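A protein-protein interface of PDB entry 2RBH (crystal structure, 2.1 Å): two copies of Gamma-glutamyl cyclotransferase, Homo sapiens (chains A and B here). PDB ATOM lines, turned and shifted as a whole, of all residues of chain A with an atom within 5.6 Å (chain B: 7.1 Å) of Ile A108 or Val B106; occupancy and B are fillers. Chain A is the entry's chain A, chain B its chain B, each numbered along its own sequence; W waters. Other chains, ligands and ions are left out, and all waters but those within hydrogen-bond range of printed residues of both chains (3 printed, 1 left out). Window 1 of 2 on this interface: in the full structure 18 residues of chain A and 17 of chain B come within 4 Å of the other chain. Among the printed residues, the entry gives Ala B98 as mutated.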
ATOM      1  N   PHE A  49     -17.937 -26.561 -12.066  1.00  0.00           N
ATOM      2  CA  PHE A  49     -18.071 -25.217 -12.606  1.00  0.00           C
ATOM      3  C   PHE A  49     -19.537 -24.821 -12.606  1.00  0.00           C
ATOM      4  O   PHE A  49     -20.430 -25.674 -12.745  1.00  0.00           O
ATOM      5  CB  PHE A  49     -17.565 -25.153 -14.040  1.00  0.00           C
ATOM      6  CG  PHE A  49     -16.081 -24.894 -14.178  1.00  0.00           C
ATOM      7  CD1 PHE A  49     -15.156 -25.924 -13.999  1.00  0.00           C
ATOM      8  CD2 PHE A  49     -15.618 -23.641 -14.559  1.00  0.00           C
ATOM      9  CE1 PHE A  49     -13.796 -25.703 -14.193  1.00  0.00           C
ATOM     10  CE2 PHE A  49     -14.246 -23.405 -14.745  1.00  0.00           C
ATOM     11  CZ  PHE A  49     -13.342 -24.439 -14.578  1.00  0.00           C
ATOM     12  N   ILE A  71     -18.348 -18.928 -16.956  1.00  0.00           N
ATOM     13  CA  ILE A  71     -18.279 -20.011 -15.988  1.00  0.00           C
ATOM     14  C   ILE A  71     -17.220 -19.725 -14.944  1.00  0.00           C
ATOM     15  O   ILE A  71     -16.230 -19.037 -15.222  1.00  0.00           O
ATOM     16  CB  ILE A  71     -18.007 -21.402 -16.652  1.00  0.00           C
ATOM     17  CG1 ILE A  71     -16.679 -21.412 -17.429  1.00  0.00           C
ATOM     18  CG2 ILE A  71     -19.194 -21.830 -17.530  1.00  0.00           C
ATOM     19  CD1 ILE A  71     -16.454 -22.657 -18.244  1.00  0.00           C
ATOM     20  N   GLN A  73     -15.280 -21.732 -11.236  1.00  0.00           N
ATOM     21  CA  GLN A  73     -15.098 -22.945 -10.452  1.00  0.00           C
ATOM     22  C   GLN A  73     -15.964 -22.922  -9.185  1.00  0.00           C
ATOM     23  O   GLN A  73     -15.966 -21.940  -8.410  1.00  0.00           O
ATOM     24  CB  GLN A  73     -13.608 -23.180 -10.151  1.00  0.00           C
ATOM     25  CG  GLN A  73     -12.774 -23.506 -11.406  1.00  0.00           C
ATOM     26  CD  GLN A  73     -11.274 -23.147 -11.294  1.00  0.00           C
ATOM     27  OE1 GLN A  73     -10.908 -22.007 -11.002  1.00  0.00           O
ATOM     28  NE2 GLN A  73     -10.414 -24.117 -11.573  1.00  0.00           N
ATOM     29  N   VAL A 106     -10.933 -14.670 -21.108  1.00  0.00           N
ATOM     30  CA  VAL A 106      -9.598 -15.224 -21.154  1.00  0.00           C
ATOM     31  C   VAL A 106      -9.702 -16.636 -21.759  1.00  0.00           C
ATOM     32  O   VAL A 106     -10.728 -17.284 -21.603  1.00  0.00           O
ATOM     33  CB  VAL A 106      -8.951 -15.253 -19.727  1.00  0.00           C
ATOM     34  CG1 VAL A 106      -9.563 -16.350 -18.865  1.00  0.00           C
ATOM     35  CG2 VAL A 106      -7.458 -15.411 -19.810  1.00  0.00           C
ATOM     36  N   VAL A 107      -8.660 -17.076 -22.481  1.00  0.00           N
ATOM     37  CA  VAL A 107      -8.595 -18.425 -23.016  1.00  0.00           C
ATOM     38  C   VAL A 107      -8.317 -19.366 -21.841  1.00  0.00           C
ATOM     39  O   VAL A 107      -7.436 -19.083 -21.026  1.00  0.00           O
ATOM     40  CB  VAL A 107      -7.460 -18.569 -24.072  1.00  0.00           C
ATOM     41  CG1 VAL A 107      -7.245 -20.029 -24.451  1.00  0.00           C
ATOM     42  CG2 VAL A 107      -7.708 -17.688 -25.300  1.00  0.00           C
ATOM     43  N   ILE A 108      -9.076 -20.459 -21.743  1.00  0.00           N
ATOM     44  CA  ILE A 108      -8.803 -21.498 -20.747  1.00  0.00           C
ATOM     45  C   ILE A 108      -8.587 -22.855 -21.422  1.00  0.00           C
ATOM     46  O   ILE A 108      -8.879 -23.027 -22.613  1.00  0.00           O
ATOM     47  CB  ILE A 108      -9.938 -21.619 -19.660  1.00  0.00           C
ATOM     48  CG1 ILE A 108     -11.306 -21.929 -20.288  1.00  0.00           C
ATOM     49  CG2 ILE A 108     -10.021 -20.357 -18.783  1.00  0.00           C
ATOM     50  CD1 ILE A 108     -12.414 -22.213 -19.230  1.00  0.00           C
ATOM     51  N   GLU A 109      -8.069 -23.796 -20.640  1.00  0.00           N
ATOM     52  CA  GLU A 109      -8.103 -25.215 -20.967  1.00  0.00           C
ATOM     53  C   GLU A 109      -8.965 -25.901 -19.929  1.00  0.00           C
ATOM     54  O   GLU A 109      -8.856 -25.629 -18.732  1.00  0.00           O
ATOM     55  CB  GLU A 109      -6.689 -25.816 -20.952  1.00  0.00           C
ATOM     56  CG  GLU A 109      -6.604 -27.231 -21.471  1.00  0.00           C
ATOM     57  CD  GLU A 109      -5.293 -27.897 -21.125  1.00  0.00           C
ATOM     58  OE1 GLU A 109      -4.298 -27.618 -21.806  1.00  0.00           O
ATOM     59  OE2 GLU A 109      -5.247 -28.686 -20.166  1.00  0.00           O
ATOM     60  N   VAL A 110      -9.823 -26.796 -20.389  1.00  0.00           N
ATOM     61  CA  VAL A 110     -10.679 -27.567 -19.492  1.00  0.00           C
ATOM     62  C   VAL A 110     -10.643 -29.030 -19.900  1.00  0.00           C
ATOM     63  O   VAL A 110     -10.325 -29.362 -21.052  1.00  0.00           O
ATOM     64  CB  VAL A 110     -12.141 -27.043 -19.479  1.00  0.00           C
ATOM     65  CG1 VAL A 110     -12.254 -25.752 -18.632  1.00  0.00           C
ATOM     66  CG2 VAL A 110     -12.654 -26.816 -20.897  1.00  0.00           C
ATOM     67  N   CYS A 122     -10.201 -29.598 -23.915  1.00  0.00           N
ATOM     68  CA  CYS A 122     -10.810 -28.593 -24.796  1.00  0.00           C
ATOM     69  C   CYS A 122     -10.332 -27.172 -24.537  1.00  0.00           C
ATOM     70  O   CYS A 122      -9.999 -26.819 -23.404  1.00  0.00           O
ATOM     71  CB  CYS A 122     -12.314 -28.590 -24.581  1.00  0.00           C
ATOM     72  SG  CYS A 122     -13.109 -30.120 -24.989  1.00  0.00           S
ATOM     73  N   ARG A 123     -10.338 -26.350 -25.578  1.00  0.00           N
ATOM     74  CA  ARG A 123     -10.140 -24.910 -25.423  1.00  0.00           C
ATOM     75  C   ARG A 123     -11.503 -24.346 -25.102  1.00  0.00           C
ATOM     76  O   ARG A 123     -12.505 -24.809 -25.653  1.00  0.00           O
ATOM     77  CB  ARG A 123      -9.597 -24.283 -26.728  1.00  0.00           C
ATOM     78  CG  ARG A 123      -9.210 -22.765 -26.642  1.00  0.00           C
ATOM     79  CD  ARG A 123      -8.816 -22.258 -28.022  1.00  0.00           C
ATOM     80  NE  ARG A 123      -8.068 -20.996 -28.049  1.00  0.00           N
ATOM     81  CZ  ARG A 123      -6.753 -20.893 -27.857  1.00  0.00           C
ATOM     82  NH1 ARG A 123      -6.037 -21.970 -27.563  1.00  0.00           N
ATOM     83  NH2 ARG A 123      -6.151 -19.709 -27.930  1.00  0.00           N
ATOM     84  N   SER A 124     -11.556 -23.382 -24.183  1.00  0.00           N
ATOM     85  CA  SER A 124     -12.785 -22.657 -23.904  1.00  0.00           C
ATOM     86  C   SER A 124     -12.420 -21.232 -23.462  1.00  0.00           C
ATOM     87  O   SER A 124     -11.277 -20.777 -23.640  1.00  0.00           O
ATOM     88  CB  SER A 124     -13.660 -23.388 -22.857  1.00  0.00           C
ATOM     89  OG  SER A 124     -15.034 -22.966 -22.896  1.00  0.00           O
ATOM     90  N   TYR A 125     -13.409 -20.527 -22.930  1.00  0.00           N
ATOM     91  CA  TYR A 125     -13.242 -19.160 -22.473  1.00  0.00           C
ATOM     92  C   TYR A 125     -14.067 -18.926 -21.202  1.00  0.00           C
ATOM     93  O   TYR A 125     -15.115 -19.559 -20.995  1.00  0.00           O
ATOM     94  CB  TYR A 125     -13.666 -18.175 -23.579  1.00  0.00           C
ATOM     95  CG  TYR A 125     -12.976 -18.409 -24.914  1.00  0.00           C
ATOM     96  CD1 TYR A 125     -11.815 -17.728 -25.241  1.00  0.00           C
ATOM     97  CD2 TYR A 125     -13.472 -19.334 -25.836  1.00  0.00           C
ATOM     98  CE1 TYR A 125     -11.151 -17.953 -26.452  1.00  0.00           C
ATOM     99  CE2 TYR A 125     -12.818 -19.558 -27.052  1.00  0.00           C
ATOM    100  CZ  TYR A 125     -11.649 -18.864 -27.336  1.00  0.00           C
ATOM    101  OH  TYR A 125     -10.983 -19.036 -28.523  1.00  0.00           O
ATOM    102  N   LEU A 126     -13.592 -18.009 -20.356  1.00  0.00           N
ATOM    103  CA  LEU A 126     -14.432 -17.436 -19.297  1.00  0.00           C
ATOM    104  C   LEU A 126     -14.059 -15.971 -19.010  1.00  0.00           C
ATOM    105  O   LEU A 126     -12.986 -15.514 -19.399  1.00  0.00           O
ATOM    106  CB  LEU A 126     -14.399 -18.309 -18.032  1.00  0.00           C
ATOM    107  CG  LEU A 126     -13.123 -18.641 -17.228  1.00  0.00           C
ATOM    108  CD1 LEU A 126     -12.666 -17.474 -16.373  1.00  0.00           C
ATOM    109  CD2 LEU A 126     -13.405 -19.819 -16.306  1.00  0.00           C
ATOM    110  N   ALA B  98      -0.862 -26.451  -9.045  1.00  0.00           N
ATOM    111  CA  ALA B  98      -1.738 -25.272  -9.044  1.00  0.00           C
ATOM    112  C   ALA B  98      -3.137 -25.528  -8.444  1.00  0.00           C
ATOM    113  O   ALA B  98      -3.904 -24.590  -8.257  1.00  0.00           O
ATOM    114  CB  ALA B  98      -1.853 -24.696 -10.461  1.00  0.00           C
ATOM    115  N   GLY B  99      -3.470 -26.786  -8.159  1.00  0.00           N
ATOM    116  CA  GLY B  99      -4.764 -27.123  -7.574  1.00  0.00           C
ATOM    117  C   GLY B  99      -5.949 -27.080  -8.527  1.00  0.00           C
ATOM    118  O   GLY B  99      -7.067 -26.711  -8.139  1.00  0.00           O
ATOM    119  N   VAL B 100      -5.706 -27.459  -9.774  1.00  0.00           N
ATOM    120  CA  VAL B 100      -6.741 -27.435 -10.802  1.00  0.00           C
ATOM    121  C   VAL B 100      -7.938 -28.335 -10.447  1.00  0.00           C
ATOM    122  O   VAL B 100      -9.081 -27.860 -10.446  1.00  0.00           O
ATOM    123  CB  VAL B 100      -6.166 -27.757 -12.216  1.00  0.00           C
ATOM    124  CG1 VAL B 100      -7.289 -27.900 -13.251  1.00  0.00           C
ATOM    125  CG2 VAL B 100      -5.181 -26.665 -12.655  1.00  0.00           C
ATOM    126  N   GLY B 103     -10.322 -27.051  -7.855  1.00  0.00           N
ATOM    127  CA  GLY B 103     -10.960 -25.786  -8.176  1.00  0.00           C
ATOM    128  C   GLY B 103     -10.227 -24.532  -7.762  1.00  0.00           C
ATOM    129  O   GLY B 103     -10.793 -23.441  -7.865  1.00  0.00           O
ATOM    130  N   MET B 104      -8.974 -24.684  -7.313  1.00  0.00           N
ATOM    131  CA  MET B 104      -8.143 -23.563  -6.829  1.00  0.00           C
ATOM    132  C   MET B 104      -7.778 -22.543  -7.930  1.00  0.00           C
ATOM    133  O   MET B 104      -7.964 -21.323  -7.759  1.00  0.00           O
ATOM    134  CB  MET B 104      -6.886 -24.096  -6.129  1.00  0.00           C
ATOM    135  CG  MET B 104      -6.184 -23.086  -5.226  1.00  0.00           C
ATOM    136  SD  MET B 104      -4.846 -23.798  -4.205  1.00  0.00           S
ATOM    137  CE  MET B 104      -5.726 -25.146  -3.394  1.00  0.00           C
ATOM    138  N   TYR B 105      -7.250 -23.054  -9.046  1.00  0.00           N
ATOM    139  CA  TYR B 105      -6.959 -22.250 -10.222  1.00  0.00           C
ATOM    140  C   TYR B 105      -7.516 -22.934 -11.458  1.00  0.00           C
ATOM    141  O   TYR B 105      -7.736 -24.149 -11.443  1.00  0.00           O
ATOM    142  CB  TYR B 105      -5.450 -22.110 -10.398  1.00  0.00           C
ATOM    143  CG  TYR B 105      -4.769 -21.198  -9.408  1.00  0.00           C
ATOM    144  CD1 TYR B 105      -4.497 -21.624  -8.121  1.00  0.00           C
ATOM    145  CD2 TYR B 105      -4.370 -19.918  -9.776  1.00  0.00           C
ATOM    146  CE1 TYR B 105      -3.852 -20.796  -7.209  1.00  0.00           C
ATOM    147  CE2 TYR B 105      -3.717 -19.086  -8.880  1.00  0.00           C
ATOM    148  CZ  TYR B 105      -3.462 -19.537  -7.598  1.00  0.00           C
ATOM    149  OH  TYR B 105      -2.815 -18.741  -6.700  1.00  0.00           O
ATOM    150  N   VAL B 106      -7.753 -22.150 -12.511  1.00  0.00           N
ATOM    151  CA  VAL B 106      -8.067 -22.685 -13.841  1.00  0.00           C
ATOM    152  C   VAL B 106      -6.824 -22.568 -14.710  1.00  0.00           C
ATOM    153  O   VAL B 106      -6.020 -21.660 -14.499  1.00  0.00           O
ATOM    154  CB  VAL B 106      -9.321 -21.993 -14.514  1.00  0.00           C
ATOM    155  CG1 VAL B 106      -9.004 -20.595 -15.043  1.00  0.00           C
ATOM    156  CG2 VAL B 106      -9.875 -22.876 -15.638  1.00  0.00           C
ATOM    157  N   VAL B 107      -6.642 -23.489 -15.656  1.00  0.00           N
ATOM    158  CA  VAL B 107      -5.560 -23.337 -16.644  1.00  0.00           C
ATOM    159  C   VAL B 107      -5.906 -22.222 -17.633  1.00  0.00           C
ATOM    160  O   VAL B 107      -7.013 -22.195 -18.170  1.00  0.00           O
ATOM    161  CB  VAL B 107      -5.330 -24.607 -17.456  1.00  0.00           C
ATOM    162  CG1 VAL B 107      -4.342 -24.333 -18.587  1.00  0.00           C
ATOM    163  CG2 VAL B 107      -4.837 -25.773 -16.572  1.00  0.00           C
ATOM    164  N   ILE B 108      -4.961 -21.318 -17.896  1.00  0.00           N
ATOM    165  CA  ILE B 108      -5.167 -20.314 -18.953  1.00  0.00           C
ATOM    166  C   ILE B 108      -4.093 -20.341 -20.048  1.00  0.00           C
ATOM    167  O   ILE B 108      -3.046 -20.965 -19.912  1.00  0.00           O
ATOM    168  CB  ILE B 108      -5.311 -18.865 -18.385  1.00  0.00           C
ATOM    169  CG1 ILE B 108      -4.005 -18.398 -17.711  1.00  0.00           C
ATOM    170  CG2 ILE B 108      -6.523 -18.775 -17.455  1.00  0.00           C
ATOM    171  CD1 ILE B 108      -4.010 -16.941 -17.290  1.00  0.00           C
ATOM    172  N   GLU B 109      -4.380 -19.659 -21.142  1.00  0.00           N
ATOM    173  CA  GLU B 109      -3.372 -19.379 -22.155  1.00  0.00           C
ATOM    174  C   GLU B 109      -3.281 -17.868 -22.243  1.00  0.00           C
ATOM    175  O   GLU B 109      -4.287 -17.196 -22.371  1.00  0.00           O
ATOM    176  CB  GLU B 109      -3.774 -19.996 -23.515  1.00  0.00           C
ATOM    177  CG  GLU B 109      -2.801 -19.732 -24.650  1.00  0.00           C
ATOM    178  CD  GLU B 109      -3.252 -20.353 -25.976  1.00  0.00           C
ATOM    179  OE1 GLU B 109      -3.140 -21.588 -26.168  1.00  0.00           O
ATOM    180  OE2 GLU B 109      -3.697 -19.594 -26.842  1.00  0.00           O
ATOM    181  N   SER B 124      -0.633 -20.593 -18.171  1.00  0.00           N
ATOM    182  CA  SER B 124      -0.566 -20.008 -16.842  1.00  0.00           C
ATOM    183  C   SER B 124      -1.823 -20.411 -16.075  1.00  0.00           C
ATOM    184  O   SER B 124      -2.537 -21.316 -16.504  1.00  0.00           O
ATOM    185  CB  SER B 124      -0.372 -18.485 -16.920  1.00  0.00           C
ATOM    186  OG  SER B 124      -0.109 -17.954 -15.626  1.00  0.00           O
ATOM    187  N   TYR B 125      -2.070 -19.771 -14.932  1.00  0.00           N
ATOM    188  CA  TYR B 125      -3.170 -20.138 -14.055  1.00  0.00           C
ATOM    189  C   TYR B 125      -3.754 -18.879 -13.410  1.00  0.00           C
ATOM    190  O   TYR B 125      -3.037 -17.921 -13.177  1.00  0.00           O
ATOM    191  CB  TYR B 125      -2.671 -21.089 -12.955  1.00  0.00           C
ATOM    192  CG  TYR B 125      -2.012 -22.347 -13.493  1.00  0.00           C
ATOM    193  CD1 TYR B 125      -2.759 -23.506 -13.728  1.00  0.00           C
ATOM    194  CD2 TYR B 125      -0.644 -22.384 -13.764  1.00  0.00           C
ATOM    195  CE1 TYR B 125      -2.153 -24.667 -14.224  1.00  0.00           C
ATOM    196  CE2 TYR B 125      -0.046 -23.541 -14.274  1.00  0.00           C
ATOM    197  CZ  TYR B 125      -0.807 -24.668 -14.497  1.00  0.00           C
ATOM    198  OH  TYR B 125      -0.220 -25.814 -14.992  1.00  0.00           O
ATOM    199  N   LEU B 126      -5.049 -18.888 -13.132  1.00  0.00           N
ATOM    200  CA  LEU B 126      -5.677 -17.806 -12.379  1.00  0.00           C
ATOM    201  C   LEU B 126      -6.867 -18.359 -11.608  1.00  0.00           C
ATOM    202  O   LEU B 126      -7.397 -19.428 -11.959  1.00  0.00           O
ATOM    203  CB  LEU B 126      -6.069 -16.619 -13.290  1.00  0.00           C
ATOM    204  CG  LEU B 126      -7.027 -16.729 -14.492  1.00  0.00           C
ATOM    205  CD1 LEU B 126      -8.472 -16.978 -14.118  1.00  0.00           C
ATOM    206  CD2 LEU B 126      -6.941 -15.445 -15.315  1.00  0.00           C
ATOM    207  N   MET B 127      -7.267 -17.651 -10.551  1.00  0.00           N
ATOM    208  CA  MET B 127      -8.399 -18.086  -9.743  1.00  0.00           C
ATOM    209  C   MET B 127      -9.685 -17.549 -10.345  1.00  0.00           C
ATOM    210  O   MET B 127      -9.708 -16.444 -10.879  1.00  0.00           O
ATOM    211  CB  MET B 127      -8.277 -17.614  -8.300  1.00  0.00           C
ATOM    212  CG  MET B 127      -7.020 -18.087  -7.598  1.00  0.00           C
ATOM    213  SD  MET B 127      -7.018 -17.690  -5.842  1.00  0.00           S
ATOM    214  CE  MET B 127      -6.717 -15.951  -5.874  1.00  0.00           C
ATOM    215  N   THR B 128     -10.755 -18.324 -10.238  1.00  0.00           N
ATOM    216  CA  THR B 128     -12.030 -17.914 -10.822  1.00  0.00           C
ATOM    217  C   THR B 128     -13.055 -17.587  -9.751  1.00  0.00           C
ATOM    218  O   THR B 128     -14.030 -16.875  -9.998  1.00  0.00           O
ATOM    219  CB  THR B 128     -12.577 -18.968 -11.803  1.00  0.00           C
ATOM    220  OG1 THR B 128     -12.802 -20.202 -11.118  1.00  0.00           O
ATOM    221  CG2 THR B 128     -11.590 -19.197 -12.933  1.00  0.00           C
HETATM  222  O   HOH W   1     -11.060 -26.858 -12.053  1.00  0.00           O
HETATM  223  O   HOH W   2      -6.233 -15.450 -23.095  1.00  0.00           O
HETATM  224  O   HOH W   3      -8.126 -25.824 -16.062  1.00  0.00           O
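Val A107 touches Ile B108, and with the chains exchanged Ile A108 touches Val B107. Val A107 touches Glu B109, and with the chains exchanged Glu A109 touches Val B107. Ile A108 touches Val B106, but with the chains exchanged Val A106 does not touch Ile B108 (4.1 Å). Positions printed for both chains: 106, 107, 108, 109, 124, 125 and 126.
Among the printed residues, pairs that only touch across the chains: Phe A49 with Val B106, Val A107 with Ile B108, Ile A108 with Val B106, Ile A108 with Val B107 and Leu A126 with Thr B128.
Printed residues of chain A that touch a printed residue of chain B: Phe A49, Gln A73, Val A107, Ile A108, Glu A109, Arg A123 and Leu A126. Of the 15 printed residues of chain B, 7 touch a printed residue of chain A. Among the printed residues, Asp or Glu carboxylates within 4 Å of a Lys or Arg side-chain nitrogen of the other chain: Arg A123 with Glu B109.
The backbone NH (N) of Glu A109 is in hydrogen-bond range of the backbone carbonyl oxygen (O) of Val B107 (3.1 Å). OE2 of Glu B109 is in salt-bridge range of NH2 of Arg A123, at 2.7 Å. The side-chain amide nitrogen (NE2) of Gln A73 lies close to the backbone NH (N) of Val B106, 3.4 Å away. The side-chain amide nitrogen of Gln A73 is in hydrogen-bond range of the backbone carbonyl oxygen of Tyr B105, 2.7 Å away. O of Gly B103 sits close to OE1 of Gln A73 (3.5 Å). The side-chain amide oxygen (OE1) of Gln A73 is in hydrogen-bond range of the side-chain hydroxyl (OG1) of Thr B128 (2.6 Å). The backbone carbonyl oxygen (O) of Val A107 lies within hydrogen-bond range of the backbone NH (N) of Glu B109, 3.1 Å away.
Water W2 bridges O of Glu B109 (2.7 Å) and N of Val A107 (3.0 Å). Water W1 lies within hydrogen-bond range of the backbone carbonyl oxygen of Val B100 and the side-chain amide nitrogen of Gln A73. Water W3 bridges O of Glu A109 and N of Val B107.
N of Val B106 is in hydrogen-bond range of O of Leu B126, at 2.8 Å. N of Ile B108 lies within hydrogen-bond range of O of Ser B124 (2.8 Å). The backbone NH of Val A106 is in hydrogen-bond range of the backbone carbonyl oxygen of Leu A126, 2.8 Å away. N of Ile A108 sits at hydrogen-bond distance from O of Ser A124 (2.9 Å).
Of the printed residues of chain B, Val A107 touches Ile B108 (3.3 Å) and Glu B109 (3.1 Å). Ile A108 touches just these residues of chain B: Val B106 (3.9 Å) and Val B107 (3.2 Å). Printed residues of chain B within 4 Å of Arg A123: Glu B109. Ser A124 touches none of the printed residues of chain B. Met B104 touches none of the printed residues of chain A. Val B106 touches three residues of chain A. The nearest residue of chain B that does not touch Ile A108 is Ile B108 (4.1 Å). The nearest residue of chain A that does not touch Val B106 is Glu A109 (4.3 Å).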
